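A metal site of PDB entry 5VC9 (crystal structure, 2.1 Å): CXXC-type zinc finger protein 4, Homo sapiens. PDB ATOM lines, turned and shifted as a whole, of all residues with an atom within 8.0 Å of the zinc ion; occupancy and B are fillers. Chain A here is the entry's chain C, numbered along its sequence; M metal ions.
The side-chain sulfur (SG) of Cys 20 lies close to the backbone NH (N) of Val 22 (3.3 Å). N of Phe 38 sits close to SG of Cys 36, at 3.5 Å. The side-chain sulfur of Cys 26 sits close to the backbone NH of Gly 21, at 3.3 Å. SG of Cys 26 lies close to NH2 of Arg 29 (3.6 Å). The side-chain sulfur (SG) of Cys 23 lies close to the backbone NH (N) of Lys 37 (3.4 Å). N of Ser 25 sits close to SG of Cys 23 (3.8 Å).
Gly 21 touches the zinc ion. Lys 37 touches the zinc ion (N to ZN, 3.98 Å). Six residues have an atom within 4 Å of the zinc ion: Cys 20, Gly 21, Cys 23, Cys 26, Cys 36 and Lys 37.
The zinc ion is bound by SG of Cys 20, 2.3 Å away. The side-chain sulfur (SG) of Cys 36 is bound to the zinc ion, at 2.3 Å. SG of Cys 26 binds the zinc ion. The zinc ion is bound by SG of Cys 23, 2.3 Å away. The zinc ion has four donor atoms within binding distance.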
ATOM      1  N   ILE A  18     -17.444  -8.367  25.875  1.00  0.00           N
ATOM      2  CA  ILE A  18     -16.982  -9.402  24.951  1.00  0.00           C
ATOM      3  C   ILE A  18     -16.772 -10.733  25.679  1.00  0.00           C
ATOM      4  O   ILE A  18     -16.100 -10.754  26.684  1.00  0.00           O
ATOM      5  CB  ILE A  18     -15.649  -8.919  24.378  1.00  0.00           C
ATOM      6  CG1 ILE A  18     -15.916  -7.857  23.318  1.00  0.00           C
ATOM      7  CG2 ILE A  18     -14.801 -10.015  23.826  1.00  0.00           C
ATOM      8  CD1 ILE A  18     -16.812  -8.323  22.200  1.00  0.00           C
ATOM      9  N   ASN A  19     -17.341 -11.810  25.121  1.00  0.00           N
ATOM     10  CA  ASN A  19     -16.992 -13.175  25.452  1.00  0.00           C
ATOM     11  C   ASN A  19     -15.505 -13.396  25.316  1.00  0.00           C
ATOM     12  O   ASN A  19     -14.917 -12.935  24.362  1.00  0.00           O
ATOM     13  CB  ASN A  19     -17.718 -14.144  24.527  1.00  0.00           C
ATOM     14  CG  ASN A  19     -19.215 -14.266  24.844  1.00  0.00           C
ATOM     15  OD1 ASN A  19     -19.655 -14.121  25.999  1.00  0.00           O
ATOM     16  ND2 ASN A  19     -19.993 -14.571  23.818  1.00  0.00           N
ATOM     17  N   CYS A  20     -14.880 -14.065  26.298  1.00  0.00           N
ATOM     18  CA  CYS A  20     -13.420 -14.233  26.293  1.00  0.00           C
ATOM     19  C   CYS A  20     -12.976 -15.199  25.135  1.00  0.00           C
ATOM     20  O   CYS A  20     -11.992 -14.955  24.436  1.00  0.00           O
ATOM     21  CB  CYS A  20     -12.865 -14.724  27.677  1.00  0.00           C
ATOM     22  SG  CYS A  20     -13.234 -16.469  28.094  1.00  0.00           S
ATOM     23  N   GLY A  21     -13.766 -16.243  24.908  1.00  0.00           N
ATOM     24  CA  GLY A  21     -13.426 -17.203  23.903  1.00  0.00           C
ATOM     25  C   GLY A  21     -12.618 -18.414  24.356  1.00  0.00           C
ATOM     26  O   GLY A  21     -12.400 -19.325  23.563  1.00  0.00           O
ATOM     27  N   VAL A  22     -12.209 -18.463  25.616  1.00  0.00           N
ATOM     28  CA  VAL A  22     -11.359 -19.555  26.095  1.00  0.00           C
ATOM     29  C   VAL A  22     -11.807 -20.234  27.416  1.00  0.00           C
ATOM     30  O   VAL A  22     -11.274 -21.274  27.776  1.00  0.00           O
ATOM     31  CB  VAL A  22      -9.904 -19.090  26.209  1.00  0.00           C
ATOM     32  CG1 VAL A  22      -9.375 -18.610  24.815  1.00  0.00           C
ATOM     33  CG2 VAL A  22      -9.738 -17.990  27.280  1.00  0.00           C
ATOM     34  N   CYS A  23     -12.796 -19.690  28.123  1.00  0.00           N
ATOM     35  CA  CYS A  23     -13.339 -20.392  29.288  1.00  0.00           C
ATOM     36  C   CYS A  23     -14.173 -21.554  28.728  1.00  0.00           C
ATOM     37  O   CYS A  23     -14.393 -21.650  27.521  1.00  0.00           O
ATOM     38  CB  CYS A  23     -14.170 -19.456  30.127  1.00  0.00           C
ATOM     39  SG  CYS A  23     -15.742 -18.996  29.330  1.00  0.00           S
ATOM     40  N   SER A  24     -14.633 -22.450  29.596  1.00  0.00           N
ATOM     41  CA  SER A  24     -15.345 -23.664  29.106  1.00  0.00           C
ATOM     42  C   SER A  24     -16.732 -23.321  28.523  1.00  0.00           C
ATOM     43  O   SER A  24     -17.147 -23.920  27.476  1.00  0.00           O
ATOM     44  CB  SER A  24     -15.465 -24.692  30.197  1.00  0.00           C
ATOM     45  OG  SER A  24     -16.215 -24.148  31.224  1.00  0.00           O
ATOM     46  N   SER A  25     -17.432 -22.369  29.162  1.00  0.00           N
ATOM     47  CA  SER A  25     -18.670 -21.836  28.595  1.00  0.00           C
ATOM     48  C   SER A  25     -18.497 -21.375  27.191  1.00  0.00           C
ATOM     49  O   SER A  25     -19.223 -21.837  26.318  1.00  0.00           O
ATOM     50  CB  SER A  25     -19.240 -20.718  29.419  1.00  0.00           C
ATOM     51  OG  SER A  25     -19.622 -21.222  30.659  1.00  0.00           O
ATOM     52  N   CYS A  26     -17.500 -20.491  26.931  1.00  0.00           N
ATOM     53  CA  CYS A  26     -17.205 -20.057  25.578  1.00  0.00           C
ATOM     54  C   CYS A  26     -16.850 -21.239  24.614  1.00  0.00           C
ATOM     55  O   CYS A  26     -17.384 -21.320  23.494  1.00  0.00           O
ATOM     56  CB  CYS A  26     -16.094 -18.980  25.562  1.00  0.00           C
ATOM     57  SG  CYS A  26     -16.612 -17.322  26.205  1.00  0.00           S
ATOM     58  N   ARG A  27     -15.982 -22.142  25.035  1.00  0.00           N
ATOM     59  CA  ARG A  27     -15.502 -23.214  24.102  1.00  0.00           C
ATOM     60  C   ARG A  27     -16.612 -24.151  23.761  1.00  0.00           C
ATOM     61  O   ARG A  27     -16.680 -24.670  22.654  1.00  0.00           O
ATOM     62  CB  ARG A  27     -14.312 -23.965  24.727  1.00  0.00           C
ATOM     63  CG  ARG A  27     -13.093 -23.046  24.861  1.00  0.00           C
ATOM     64  CD  ARG A  27     -11.762 -23.770  25.201  1.00  0.00           C
ATOM     65  NE  ARG A  27     -11.713 -24.350  26.590  1.00  0.00           N
ATOM     66  CZ  ARG A  27     -12.068 -25.615  26.943  1.00  0.00           C
ATOM     67  NH1 ARG A  27     -12.529 -26.521  26.030  1.00  0.00           N
ATOM     68  NH2 ARG A  27     -11.967 -25.972  28.222  1.00  0.00           N
ATOM     69  N   ARG A  29     -19.874 -23.413  23.612  1.00  0.00           N
ATOM     70  CA  ARG A  29     -21.092 -22.577  23.440  1.00  0.00           C
ATOM     71  C   ARG A  29     -22.138 -23.207  22.535  1.00  0.00           C
ATOM     72  O   ARG A  29     -23.302 -23.158  22.851  1.00  0.00           O
ATOM     73  CB  ARG A  29     -20.739 -21.144  22.950  1.00  0.00           C
ATOM     74  CG  ARG A  29     -21.942 -20.306  22.529  1.00  0.00           C
ATOM     75  CD  ARG A  29     -21.607 -18.825  22.438  1.00  0.00           C
ATOM     76  NE  ARG A  29     -21.422 -18.393  23.801  1.00  0.00           N
ATOM     77  CZ  ARG A  29     -20.258 -18.071  24.381  1.00  0.00           C
ATOM     78  NH1 ARG A  29     -20.272 -17.763  25.686  1.00  0.00           N
ATOM     79  NH2 ARG A  29     -19.079 -18.085  23.676  1.00  0.00           N
ATOM     80  N   GLN A  34     -24.170 -21.318  26.973  1.00  0.00           N
ATOM     81  CA  GLN A  34     -23.999 -20.484  28.198  1.00  0.00           C
ATOM     82  C   GLN A  34     -23.155 -19.237  27.863  1.00  0.00           C
ATOM     83  O   GLN A  34     -22.237 -19.288  27.079  1.00  0.00           O
ATOM     84  CB  GLN A  34     -23.317 -21.246  29.366  1.00  0.00           C
ATOM     85  CG  GLN A  34     -24.006 -22.542  29.850  1.00  0.00           C
ATOM     86  CD  GLN A  34     -25.484 -22.330  30.264  1.00  0.00           C
ATOM     87  OE1 GLN A  34     -25.815 -21.495  31.123  1.00  0.00           O
ATOM     88  NE2 GLN A  34     -26.370 -23.150  29.683  1.00  0.00           N
ATOM     89  N   ILE A  35     -23.481 -18.161  28.521  1.00  0.00           N
ATOM     90  CA  ILE A  35     -22.656 -16.946  28.509  1.00  0.00           C
ATOM     91  C   ILE A  35     -21.253 -17.225  29.058  1.00  0.00           C
ATOM     92  O   ILE A  35     -21.067 -18.118  29.836  1.00  0.00           O
ATOM     93  CB  ILE A  35     -23.367 -15.796  29.321  1.00  0.00           C
ATOM     94  CG1 ILE A  35     -22.758 -14.439  29.019  1.00  0.00           C
ATOM     95  CG2 ILE A  35     -23.295 -16.080  30.798  1.00  0.00           C
ATOM     96  CD1 ILE A  35     -23.640 -13.290  29.441  1.00  0.00           C
ATOM     97  N   CYS A  36     -20.274 -16.480  28.578  1.00  0.00           N
ATOM     98  CA  CYS A  36     -18.913 -16.484  29.082  1.00  0.00           C
ATOM     99  C   CYS A  36     -18.869 -16.434  30.599  1.00  0.00           C
ATOM    100  O   CYS A  36     -19.591 -15.643  31.211  1.00  0.00           O
ATOM    101  CB  CYS A  36     -18.142 -15.280  28.501  1.00  0.00           C
ATOM    102  SG  CYS A  36     -16.464 -15.079  29.078  1.00  0.00           S
ATOM    103  N   LYS A  37     -18.023 -17.270  31.214  1.00  0.00           N
ATOM    104  CA  LYS A  37     -17.930 -17.268  32.738  1.00  0.00           C
ATOM    105  C   LYS A  37     -17.619 -15.869  33.294  1.00  0.00           C
ATOM    106  O   LYS A  37     -17.996 -15.547  34.439  1.00  0.00           O
ATOM    107  CB  LYS A  37     -16.863 -18.264  33.250  1.00  0.00           C
ATOM    108  N   PHE A  38     -16.873 -15.083  32.539  1.00  0.00           N
ATOM    109  CA  PHE A  38     -16.499 -13.746  32.993  1.00  0.00           C
ATOM    110  C   PHE A  38     -17.597 -12.674  32.782  1.00  0.00           C
ATOM    111  O   PHE A  38     -17.454 -11.544  33.294  1.00  0.00           O
ATOM    112  CB  PHE A  38     -15.187 -13.293  32.325  1.00  0.00           C
ATOM    113  CG  PHE A  38     -14.032 -14.297  32.489  1.00  0.00           C
ATOM    114  CD1 PHE A  38     -13.388 -14.439  33.715  1.00  0.00           C
ATOM    115  CD2 PHE A  38     -13.593 -15.104  31.393  1.00  0.00           C
ATOM    116  CE1 PHE A  38     -12.309 -15.361  33.869  1.00  0.00           C
ATOM    117  CE2 PHE A  38     -12.514 -16.025  31.547  1.00  0.00           C
ATOM    118  CZ  PHE A  38     -11.875 -16.148  32.783  1.00  0.00           C
ATOM    119  N   ARG A  39     -18.651 -12.990  32.010  1.00  0.00           N
ATOM    120  CA  ARG A  39     -19.797 -12.039  31.794  1.00  0.00           C
ATOM    121  C   ARG A  39     -21.016 -12.441  32.565  1.00  0.00           C
ATOM    122  O   ARG A  39     -21.957 -11.639  32.682  1.00  0.00           O
ATOM    123  CB  ARG A  39     -20.166 -11.960  30.333  1.00  0.00           C
ATOM    124  CG  ARG A  39     -19.052 -11.404  29.478  1.00  0.00           C
ATOM    125  CD  ARG A  39     -19.477 -11.371  28.052  1.00  0.00           C
ATOM    126  NE  ARG A  39     -20.698 -10.567  27.852  1.00  0.00           N
ATOM    127  CZ  ARG A  39     -21.774 -10.946  27.126  1.00  0.00           C
ATOM    128  NH1 ARG A  39     -21.798 -12.109  26.480  1.00  0.00           N
ATOM    129  NH2 ARG A  39     -22.827 -10.116  26.990  1.00  0.00           N
HETATM  130 ZN    ZN M   1     -15.467 -16.966  28.184  1.00  0.00          ZN
